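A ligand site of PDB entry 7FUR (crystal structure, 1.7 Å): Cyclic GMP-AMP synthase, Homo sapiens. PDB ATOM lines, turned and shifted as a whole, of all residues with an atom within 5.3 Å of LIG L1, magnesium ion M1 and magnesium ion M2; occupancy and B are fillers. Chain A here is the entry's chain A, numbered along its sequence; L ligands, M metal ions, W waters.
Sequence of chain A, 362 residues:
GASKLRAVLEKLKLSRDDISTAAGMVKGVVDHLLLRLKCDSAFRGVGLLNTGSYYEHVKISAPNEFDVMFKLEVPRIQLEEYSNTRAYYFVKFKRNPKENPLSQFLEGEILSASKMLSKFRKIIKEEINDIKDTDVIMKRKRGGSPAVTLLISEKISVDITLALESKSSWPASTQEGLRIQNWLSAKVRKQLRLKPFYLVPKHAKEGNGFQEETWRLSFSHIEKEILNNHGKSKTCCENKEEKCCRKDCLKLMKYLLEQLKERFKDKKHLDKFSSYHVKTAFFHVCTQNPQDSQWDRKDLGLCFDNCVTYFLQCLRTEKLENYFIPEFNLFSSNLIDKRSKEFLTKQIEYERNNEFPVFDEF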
ATOM      1  N   THR A  51      27.172   9.217  20.506  1.00  0.00           N
ATOM      2  CA  THR A  51      27.997  10.398  20.767  1.00  0.00           C
ATOM      3  C   THR A  51      27.228  11.398  21.639  1.00  0.00           C
ATOM      4  O   THR A  51      26.047  11.215  21.959  1.00  0.00           O
ATOM      5  CB  THR A  51      28.407  11.070  19.459  1.00  0.00           C
ATOM      6  OG1 THR A  51      27.206  11.482  18.787  1.00  0.00           O
ATOM      7  CG2 THR A  51      29.193  10.127  18.564  1.00  0.00           C
ATOM      8  N   GLY A  52      27.904  12.503  21.978  1.00  0.00           N
ATOM      9  CA  GLY A  52      27.223  13.574  22.680  1.00  0.00           C
ATOM     10  C   GLY A  52      27.066  13.281  24.155  1.00  0.00           C
ATOM     11  O   GLY A  52      27.535  12.260  24.681  1.00  0.00           O
ATOM     12  N   SER A  53      26.369  14.196  24.835  1.00  0.00           N
ATOM     13  CA  SER A  53      26.447  14.287  26.284  1.00  0.00           C
ATOM     14  C   SER A  53      25.802  13.098  27.006  1.00  0.00           C
ATOM     15  O   SER A  53      26.239  12.746  28.109  1.00  0.00           O
ATOM     16  CB  SER A  53      25.803  15.585  26.754  1.00  0.00           C
ATOM     17  OG  SER A  53      24.393  15.574  26.540  1.00  0.00           O
ATOM     18  N   TYR A  54      24.743  12.501  26.451  1.00  0.00           N
ATOM     19  CA  TYR A  54      24.154  11.358  27.143  1.00  0.00           C
ATOM     20  C   TYR A  54      25.167  10.224  27.283  1.00  0.00           C
ATOM     21  O   TYR A  54      25.299   9.636  28.362  1.00  0.00           O
ATOM     22  CB  TYR A  54      22.909  10.840  26.412  1.00  0.00           C
ATOM     23  CG  TYR A  54      22.302   9.600  27.066  1.00  0.00           C
ATOM     24  CD1 TYR A  54      21.494   9.706  28.190  1.00  0.00           C
ATOM     25  CD2 TYR A  54      22.510   8.324  26.534  1.00  0.00           C
ATOM     26  CE1 TYR A  54      20.934   8.578  28.770  1.00  0.00           C
ATOM     27  CE2 TYR A  54      21.962   7.201  27.120  1.00  0.00           C
ATOM     28  CZ  TYR A  54      21.174   7.328  28.238  1.00  0.00           C
ATOM     29  OH  TYR A  54      20.598   6.202  28.800  1.00  0.00           O
ATOM     30  N   GLU A  56      28.416  10.377  27.042  1.00  0.00           N
ATOM     31  CA  GLU A  56      29.545  10.853  27.845  1.00  0.00           C
ATOM     32  C   GLU A  56      29.186  11.029  29.318  1.00  0.00           C
ATOM     33  O   GLU A  56      30.073  11.348  30.118  1.00  0.00           O
ATOM     34  CB  GLU A  56      30.022  12.186  27.295  1.00  0.00           C
ATOM     35  CG  GLU A  56      30.494  12.084  25.863  1.00  0.00           C
ATOM     36  CD  GLU A  56      30.586  13.451  25.218  1.00  0.00           C
ATOM     37  OE1 GLU A  56      29.917  14.383  25.716  1.00  0.00           O
ATOM     38  OE2 GLU A  56      31.333  13.577  24.221  1.00  0.00           O
ATOM     39  N   VAL A  58      27.402  13.358  30.749  1.00  0.00           N
ATOM     40  CA  VAL A  58      27.356  14.749  31.238  1.00  0.00           C
ATOM     41  C   VAL A  58      26.074  15.452  30.821  1.00  0.00           C
ATOM     42  O   VAL A  58      25.937  16.666  31.020  1.00  0.00           O
ATOM     43  CB  VAL A  58      28.589  15.575  30.789  1.00  0.00           C
ATOM     44  CG1 VAL A  58      29.873  15.041  31.447  1.00  0.00           C
ATOM     45  CG2 VAL A  58      28.717  15.633  29.266  1.00  0.00           C
ATOM     46  N   LYS A  59      25.119  14.706  30.258  1.00  0.00           N
ATOM     47  CA  LYS A  59      23.778  15.260  30.054  1.00  0.00           C
ATOM     48  C   LYS A  59      23.192  15.706  31.387  1.00  0.00           C
ATOM     49  O   LYS A  59      23.233  14.966  32.375  1.00  0.00           O
ATOM     50  CB  LYS A  59      22.852  14.212  29.410  1.00  0.00           C
ATOM     51  CG  LYS A  59      21.435  14.739  29.068  1.00  0.00           C
ATOM     52  CD  LYS A  59      21.460  15.515  27.747  1.00  0.00           C
ATOM     53  CE  LYS A  59      20.114  16.200  27.467  1.00  0.00           C
ATOM     54  NZ  LYS A  59      19.717  17.217  28.520  1.00  0.00           N
ATOM     55  N   ILE A  60      22.644  16.927  31.442  1.00  0.00           N
ATOM     56  CA  ILE A  60      22.121  17.481  32.688  1.00  0.00           C
ATOM     57  C   ILE A  60      20.601  17.588  32.604  1.00  0.00           C
ATOM     58  O   ILE A  60      20.006  17.628  31.525  1.00  0.00           O
ATOM     59  CB  ILE A  60      22.721  18.864  32.995  1.00  0.00           C
ATOM     60  CG1 ILE A  60      22.417  19.808  31.831  1.00  0.00           C
ATOM     61  CG2 ILE A  60      24.234  18.747  33.227  1.00  0.00           C
ATOM     62  CD1 ILE A  60      22.761  21.242  32.083  1.00  0.00           C
ATOM     63  N   GLU A  65      17.549  14.544  25.080  1.00  0.00           N
ATOM     64  CA  GLU A  65      18.252  14.862  23.838  1.00  0.00           C
ATOM     65  C   GLU A  65      19.398  13.886  23.631  1.00  0.00           C
ATOM     66  O   GLU A  65      20.311  13.801  24.461  1.00  0.00           O
ATOM     67  CB  GLU A  65      18.781  16.303  23.836  1.00  0.00           C
ATOM     68  CG  GLU A  65      18.983  16.862  22.423  1.00  0.00           C
ATOM     69  CD  GLU A  65      20.413  16.721  21.888  1.00  0.00           C
ATOM     70  OE1 GLU A  65      21.326  16.278  22.616  1.00  0.00           O
ATOM     71  OE2 GLU A  65      20.622  17.078  20.702  1.00  0.00           O
ATOM     72  N   PHE A  66      19.369  13.182  22.497  1.00  0.00           N
ATOM     73  CA  PHE A  66      20.346  12.150  22.200  1.00  0.00           C
ATOM     74  C   PHE A  66      21.010  12.466  20.868  1.00  0.00           C
ATOM     75  O   PHE A  66      20.373  13.004  19.962  1.00  0.00           O
ATOM     76  CB  PHE A  66      19.705  10.765  22.131  1.00  0.00           C
ATOM     77  CG  PHE A  66      19.136  10.287  23.430  1.00  0.00           C
ATOM     78  CD1 PHE A  66      17.991  10.872  23.985  1.00  0.00           C
ATOM     79  CD2 PHE A  66      19.717   9.219  24.094  1.00  0.00           C
ATOM     80  CE1 PHE A  66      17.451  10.401  25.177  1.00  0.00           C
ATOM     81  CE2 PHE A  66      19.179   8.739  25.290  1.00  0.00           C
ATOM     82  CZ  PHE A  66      18.040   9.328  25.829  1.00  0.00           C
ATOM     83  N   ASP A  67      22.275  12.065  20.730  1.00  0.00           N
ATOM     84  CA  ASP A  67      23.009  12.322  19.496  1.00  0.00           C
ATOM     85  C   ASP A  67      23.610  11.009  19.025  1.00  0.00           C
ATOM     86  O   ASP A  67      24.359  10.361  19.772  1.00  0.00           O
ATOM     87  CB  ASP A  67      24.114  13.369  19.705  1.00  0.00           C
ATOM     88  CG  ASP A  67      23.575  14.656  20.251  1.00  0.00           C
ATOM     89  OD1 ASP A  67      22.993  15.437  19.474  1.00  0.00           O
ATOM     90  OD2 ASP A  67      23.711  14.874  21.487  1.00  0.00           O
ATOM     91  N   ASP A 159      19.230  13.649  17.375  1.00  0.00           N
ATOM     92  CA  ASP A 159      19.973  14.081  16.204  1.00  0.00           C
ATOM     93  C   ASP A 159      20.605  12.842  15.579  1.00  0.00           C
ATOM     94  O   ASP A 159      21.354  12.131  16.240  1.00  0.00           O
ATOM     95  CB  ASP A 159      21.064  15.083  16.580  1.00  0.00           C
ATOM     96  CG  ASP A 159      20.490  16.435  16.964  1.00  0.00           C
ATOM     97  OD1 ASP A 159      19.517  16.887  16.311  1.00  0.00           O
ATOM     98  OD2 ASP A 159      21.013  17.042  17.920  1.00  0.00           O
ATOM     99  N   ARG A 216      32.359  18.338   6.691  1.00  0.00           N
ATOM    100  CA  ARG A 216      33.095  18.855   7.841  1.00  0.00           C
ATOM    101  C   ARG A 216      33.673  17.738   8.706  1.00  0.00           C
ATOM    102  O   ARG A 216      33.022  16.716   8.938  1.00  0.00           O
ATOM    103  CB  ARG A 216      32.225  19.736   8.715  1.00  0.00           C
ATOM    104  CG  ARG A 216      33.051  20.310   9.806  1.00  0.00           C
ATOM    105  CD  ARG A 216      32.317  21.259  10.634  1.00  0.00           C
ATOM    106  NE  ARG A 216      33.144  21.551  11.784  1.00  0.00           N
ATOM    107  CZ  ARG A 216      33.047  22.657  12.503  1.00  0.00           C
ATOM    108  NH1 ARG A 216      33.853  22.838  13.540  1.00  0.00           N
ATOM    109  NH2 ARG A 216      32.150  23.587  12.168  1.00  0.00           N
ATOM    110  N   SER A 220      33.841  13.512  17.256  1.00  0.00           N
ATOM    111  CA  SER A 220      32.924  13.302  18.365  1.00  0.00           C
ATOM    112  C   SER A 220      33.208  12.001  19.129  1.00  0.00           C
ATOM    113  O   SER A 220      33.039  11.942  20.351  1.00  0.00           O
ATOM    114  CB  SER A 220      31.503  13.337  17.804  1.00  0.00           C
ATOM    115  OG  SER A 220      30.542  13.475  18.835  1.00  0.00           O
ATOM    116  N   GLU A 223      36.068  12.671  21.512  1.00  0.00           N
ATOM    117  CA  GLU A 223      35.532  13.414  22.645  1.00  0.00           C
ATOM    118  C   GLU A 223      34.912  12.469  23.669  1.00  0.00           C
ATOM    119  O   GLU A 223      35.169  12.594  24.875  1.00  0.00           O
ATOM    120  CB  GLU A 223      34.520  14.459  22.152  1.00  0.00           C
ATOM    121  CG  GLU A 223      35.145  15.551  21.250  1.00  0.00           C
ATOM    122  CD  GLU A 223      34.127  16.449  20.564  1.00  0.00           C
ATOM    123  OE1 GLU A 223      32.914  16.380  20.896  1.00  0.00           O
ATOM    124  OE2 GLU A 223      34.545  17.236  19.664  1.00  0.00           O
ATOM    125  N   LYS A 254      27.886  23.551  31.747  1.00  0.00           N
ATOM    126  CA  LYS A 254      26.758  23.368  30.856  1.00  0.00           C
ATOM    127  C   LYS A 254      25.519  24.030  31.428  1.00  0.00           C
ATOM    128  O   LYS A 254      24.783  24.718  30.715  1.00  0.00           O
ATOM    129  CB  LYS A 254      26.513  21.887  30.629  1.00  0.00           C
ATOM    130  CG  LYS A 254      27.502  21.258  29.682  1.00  0.00           C
ATOM    131  CD  LYS A 254      27.382  19.751  29.730  1.00  0.00           C
ATOM    132  CE  LYS A 254      26.028  19.285  29.245  1.00  0.00           C
ATOM    133  NZ  LYS A 254      25.924  19.666  27.791  1.00  0.00           N
ATOM    134  N   SER A 274      26.498  27.630  22.472  1.00  0.00           N
ATOM    135  CA  SER A 274      26.087  26.244  22.570  1.00  0.00           C
ATOM    136  C   SER A 274      26.885  25.539  23.656  1.00  0.00           C
ATOM    137  O   SER A 274      27.945  25.996  24.106  1.00  0.00           O
ATOM    138  CB  SER A 274      26.287  25.509  21.233  1.00  0.00           C
ATOM    139  OG  SER A 274      27.640  25.107  21.076  1.00  0.00           O
ATOM    140  N   SER A 275      26.368  24.369  24.045  1.00  0.00           N
ATOM    141  CA  SER A 275      27.103  23.569  25.013  1.00  0.00           C
ATOM    142  C   SER A 275      28.469  23.163  24.492  1.00  0.00           C
ATOM    143  O   SER A 275      29.377  22.899  25.273  1.00  0.00           O
ATOM    144  CB  SER A 275      26.299  22.332  25.404  1.00  0.00           C
ATOM    145  OG  SER A 275      26.062  21.538  24.257  1.00  0.00           O
ATOM    146  N   TYR A 276      28.630  23.106  23.167  1.00  0.00           N
ATOM    147  CA  TYR A 276      29.918  22.714  22.596  1.00  0.00           C
ATOM    148  C   TYR A 276      30.996  23.740  22.859  1.00  0.00           C
ATOM    149  O   TYR A 276      32.182  23.407  22.925  1.00  0.00           O
ATOM    150  CB  TYR A 276      29.791  22.469  21.089  1.00  0.00           C
ATOM    151  CG  TYR A 276      31.008  21.777  20.552  1.00  0.00           C
ATOM    152  CD1 TYR A 276      31.267  20.452  20.870  1.00  0.00           C
ATOM    153  CD2 TYR A 276      31.913  22.449  19.720  1.00  0.00           C
ATOM    154  CE1 TYR A 276      32.379  19.811  20.390  1.00  0.00           C
ATOM    155  CE2 TYR A 276      33.008  21.817  19.217  1.00  0.00           C
ATOM    156  CZ  TYR A 276      33.243  20.512  19.557  1.00  0.00           C
ATOM    157  OH  TYR A 276      34.363  19.897  19.061  1.00  0.00           O
ATOM    158  N   LYS A 279      32.038  22.853  26.315  1.00  0.00           N
ATOM    159  CA  LYS A 279      32.765  21.581  26.237  1.00  0.00           C
ATOM    160  C   LYS A 279      34.180  21.790  25.718  1.00  0.00           C
ATOM    161  O   LYS A 279      35.141  21.227  26.256  1.00  0.00           O
ATOM    162  CB  LYS A 279      31.996  20.604  25.340  1.00  0.00           C
ATOM    163  CG  LYS A 279      32.452  19.164  25.472  1.00  0.00           C
ATOM    164  CD  LYS A 279      31.889  18.350  24.295  1.00  0.00           C
ATOM    165  CE  LYS A 279      32.006  16.841  24.461  1.00  0.00           C
ATOM    166  NZ  LYS A 279      31.323  16.102  23.322  1.00  0.00           N
ATOM    167  N   ASN A 322      39.112  25.183  18.380  1.00  0.00           N
ATOM    168  CA  ASN A 322      38.641  23.801  18.286  1.00  0.00           C
ATOM    169  C   ASN A 322      39.720  22.886  18.832  1.00  0.00           C
ATOM    170  O   ASN A 322      40.921  23.067  18.576  1.00  0.00           O
ATOM    171  CB  ASN A 322      38.293  23.471  16.828  1.00  0.00           C
ATOM    172  CG  ASN A 322      37.715  22.069  16.663  1.00  0.00           C
ATOM    173  OD1 ASN A 322      38.440  21.078  16.760  1.00  0.00           O
ATOM    174  ND2 ASN A 322      36.423  21.966  16.373  1.00  0.00           N
HETATM  175  P1  LIG L   1      23.960  18.646  25.185  1.00  0.00           P
HETATM  176  O1  LIG L   1      23.222  17.811  24.159  1.00  0.00           O
HETATM  177  O2  LIG L   1      23.763  20.119  25.005  1.00  0.00           O
HETATM  178  O3  LIG L   1      23.873  18.182  26.616  1.00  0.00           O
HETATM  179  P2  LIG L   1      26.061  17.681  23.464  1.00  0.00           P
HETATM  180  O4  LIG L   1      27.587  17.623  23.557  1.00  0.00           O
HETATM  181  O5  LIG L   1      25.350  16.391  23.184  1.00  0.00           O
HETATM  182  O6  LIG L   1      25.549  18.360  24.855  1.00  0.00           O
HETATM  183  P3  LIG L   1      24.823  18.610  20.955  1.00  0.00           P
HETATM  184  O7  LIG L   1      24.510  20.037  20.511  1.00  0.00           O
HETATM  185  O8  LIG L   1      23.751  17.556  21.054  1.00  0.00           O
HETATM  186  O9  LIG L   1      25.620  18.800  22.365  1.00  0.00           O
HETATM  187  O10 LIG L   1      25.974  18.048  19.977  1.00  0.00           O
HETATM  188  C1  LIG L   1      26.189  16.655  19.830  1.00  0.00           C
HETATM  189  C2  LIG L   1      27.649  16.507  19.393  1.00  0.00           C
HETATM  190  O11 LIG L   1      27.809  17.235  18.179  1.00  0.00           O
HETATM  191  C3  LIG L   1      28.635  17.161  20.342  1.00  0.00           C
HETATM  192  O12 LIG L   1      29.054  16.282  21.388  1.00  0.00           O
HETATM  193  C4  LIG L   1      29.796  17.481  19.423  1.00  0.00           C
HETATM  194  O13 LIG L   1      30.649  16.326  19.359  1.00  0.00           O
HETATM  195  C5  LIG L   1      29.146  17.717  18.065  1.00  0.00           C
HETATM  196  N1  LIG L   1      29.094  19.168  17.812  1.00  0.00           N
HETATM  197  C6  LIG L   1      28.103  20.012  18.137  1.00  0.00           C
HETATM  198  N2  LIG L   1      28.407  21.267  17.756  1.00  0.00           N
HETATM  199  C7  LIG L   1      29.632  21.224  17.183  1.00  0.00           C
HETATM  200  C8  LIG L   1      30.566  22.193  16.554  1.00  0.00           C
HETATM  201  N3  LIG L   1      30.238  23.500  16.491  1.00  0.00           N
HETATM  202  N4  LIG L   1      31.741  21.714  16.076  1.00  0.00           N
HETATM  203  C9  LIG L   1      32.081  20.420  16.141  1.00  0.00           C
HETATM  204  N5  LIG L   1      31.272  19.501  16.690  1.00  0.00           N
HETATM  205  C10 LIG L   1      30.080  19.834  17.211  1.00  0.00           C
HETATM  206  C1  LG2 L   2      23.845  20.559  15.741  1.00  0.00           C
HETATM  207  C2  LG2 L   2      27.577  16.117  15.122  1.00  0.00           C
HETATM  208  C3  LG2 L   2      26.267  15.751  14.794  1.00  0.00           C
HETATM  209  C4  LG2 L   2      28.299  15.215  15.900  1.00  0.00           C
HETATM  210  O1  LG2 L   2      21.861  19.285  19.325  1.00  0.00           O
HETATM  211  C5  LG2 L   2      22.393  19.922  18.181  1.00  0.00           C
HETATM  212  C6  LG2 L   2      23.440  18.980  17.617  1.00  0.00           C
HETATM  213  O2  LG2 L   2      23.664  17.935  18.204  1.00  0.00           O
HETATM  214  N1  LG2 L   2      24.098  19.327  16.493  1.00  0.00           N
HETATM  215  C7  LG2 L   2      25.089  18.411  15.946  1.00  0.00           C
HETATM  216  C8  LG2 L   2      26.254  19.142  15.334  1.00  0.00           C
HETATM  217  C9  LG2 L   2      27.543  18.665  14.817  1.00  0.00           C
HETATM  218  C10 LG2 L   2      28.200  19.821  14.375  1.00  0.00           C
HETATM  219  N2  LG2 L   2      27.394  20.924  14.602  1.00  0.00           N
HETATM  220  C11 LG2 L   2      26.226  20.497  15.179  1.00  0.00           C
HETATM  221  C12 LG2 L   2      25.105  21.390  15.583  1.00  0.00           C
HETATM  222  C13 LG2 L   2      29.478  19.752  13.809  1.00  0.00           C
HETATM  223 CL1  LG2 L   2      30.261  21.188  13.279  1.00  0.00          CL
HETATM  224  C14 LG2 L   2      30.087  18.514  13.683  1.00  0.00           C
HETATM  225 CL2  LG2 L   2      31.677  18.381  13.019  1.00  0.00          CL
HETATM  226  C15 LG2 L   2      29.458  17.365  14.112  1.00  0.00           C
HETATM  227  C16 LG2 L   2      28.176  17.407  14.669  1.00  0.00           C
HETATM  228  N3  LG2 L   2      25.683  14.616  15.199  1.00  0.00           N
HETATM  229  C17 LG2 L   2      26.390  13.747  15.955  1.00  0.00           C
HETATM  230  N4  LG2 L   2      25.781  12.605  16.349  1.00  0.00           N
HETATM  231  C18 LG2 L   2      27.729  14.026  16.328  1.00  0.00           C
HETATM  232 MG    MG M   1      23.288  16.376  22.797  1.00  0.00          MG
HETATM  233 MG    MG M   2      22.305  17.263  19.566  1.00  0.00          MG
HETATM  234  O   HOH W   1      26.563  23.059  18.693  1.00  0.00           O
HETATM  235  O   HOH W   2      28.355  19.568  26.554  1.00  0.00           O
HETATM  236  O   HOH W   3      23.127  21.149  22.555  1.00  0.00           O
HETATM  237  O   HOH W   4      28.829  17.070  26.040  1.00  0.00           O
HETATM  238  O   HOH W   5      31.909  25.822  15.470  1.00  0.00           O
HETATM  239  O   HOH W   6      22.437  18.477  28.889  1.00  0.00           O
HETATM  240  O   HOH W   7      32.230  16.817  16.421  1.00  0.00           O
HETATM  241  O   HOH W   8      27.966  25.200  18.228  1.00  0.00           O
HETATM  242  O   HOH W   9      28.464  20.113  23.764  1.00  0.00           O
HETATM  243  O   HOH W  10      23.112  14.923  24.240  1.00  0.00           O
HETATM  244  O   HOH W  11      21.691  21.186  26.091  1.00  0.00           O
HETATM  245  O   HOH W  12      33.922  23.676  16.056  1.00  0.00           O
HETATM  246  O   HOH W  13      26.302  22.004  21.229  1.00  0.00           O
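An oxygen (O3) of LIG L1 is in hydrogen-bond range of the side-chain hydroxyl (OG) of Ser 53 (2.7 Å).
The side-chain amino group (NZ) of Lys 254 lies within salt-bridge range of an oxygen (O3) of LIG L1 (2.8 Å).
O13 of LIG L1 sits at hydrogen-bond distance from OE1 of Glu 223 (2.7 Å).
OG of Ser 275 lies within hydrogen-bond range of O2 of LIG L1 (2.8 Å).
An oxygen (O13) of LIG L1 sits at hydrogen-bond distance from the side-chain hydroxyl of Ser 220 (2.9 Å).
NH1 of Arg 216 is in hydrogen-bond range of N4 of LIG L1 (3.5 Å).
OG1 of Thr 51 sits at hydrogen-bond distance from N4 of LG2 L2 (3.0 Å).
The side-chain amino group (NZ) of Lys 279 is in hydrogen-bond range of an oxygen (O12) of LIG L1 (3.0 Å).
N of Ser 53 sits close to O5 of LIG L1 (2.9 Å).
Magnesium ion M1 is bound by OE1 of Glu 65, O1 of LIG L1, OD2 of Asp 67, water W10, O5 of LIG L1 and O8 of LIG L1.
Magnesium ion M1 has six donor atoms within binding distance.
OD1 of Asp 67 is bound to magnesium ion M2 (2.0 Å).
O2 of LG2 L2 is bound to magnesium ion M2, at 2.0 Å.
OE2 of Glu 65 binds magnesium ion M2 (2.0 Å).
Magnesium ion M2 is bound by O1 of LG2 L2 (2.1 Å).
O8 of LIG L1 is bound to magnesium ion M2 (2.1 Å).
Magnesium ion M2 is bound by the side-chain carboxylate (OD2) of Asp 159 (2.1 Å).
Within 4 Å of magnesium ion M2: Glu 65, Asp 67 and Asp 159.
Gly 52 touches LIG L1.
Lys 59 touches LIG L1 (CD to O3, 3.8 Å).
Tyr 276 touches LIG L1 (CE2 to N4, 3.4 Å).
12 residues have an atom within 4 Å of LIG L1: Gly 52, Ser 53, Lys 59, Glu 65, Asp 67, Arg 216, Ser 220, Glu 223, Lys 254, Ser 275, Tyr 276 and Lys 279.
Water W10 bridges the side-chain hydroxyl of Ser 53 and the backbone carbonyl oxygen of Glu 65.
Water W6 lies within hydrogen-bond range of O3 of LIG L1, N of Ile 60 and NZ of Lys 59.
Water W3 bridges an oxygen (O7) of LIG L1 and the side-chain hydroxyl of Ser 275.
Water W13 lies within hydrogen-bond range of O7 of LIG L1, OG of Ser 275, N of Tyr 276 and OG of Ser 274.
Water W4 bridges an oxygen (O4) of LIG L1 (2.8 Å) and the side-chain carboxylate (OE1) of Glu 56 (2.9 Å).
Water W2 bridges the side-chain amino group of Lys 254 and an oxygen (O6) of LIG L1.
Merely in contact with magnesium ion M1: Ser 53 (3.98 Å).
Of the 21 residues printed, 3 come within 4 Å of magnesium ion M1.
The nearest printed residue that does not touch magnesium ion M1 is Gly 52 (4.8 Å).
The backbone NH (N) of Tyr 276 lies close to the side-chain hydroxyl (OG) of Ser 274.
The side-chain amino group of Lys 279 is in salt-bridge range of the side-chain carboxylate of Glu 223, 2.9 Å away.
The backbone carbonyl oxygen (O) of Ser 53 lies within hydrogen-bond range of the backbone NH (N) of Val 58 (2.9 Å).
N of Thr 51 lies within hydrogen-bond range of O of Asp 67 (3.1 Å).
O of Phe 66 is in hydrogen-bond range of N of Asp 159 (2.9 Å).
The side-chain hydroxyl (OH) of Tyr 276 lies within hydrogen-bond range of the side-chain carboxylate (OE2) of Glu 223 (2.7 Å).
The backbone carbonyl oxygen (O) of Ser 53 is in hydrogen-bond range of the backbone NH (N) of Lys 59 (3.1 Å).
The side-chain amino group (NZ) of Lys 279 lies within salt-bridge range of the side-chain carboxylate (OE2) of Glu 56 (2.7 Å).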
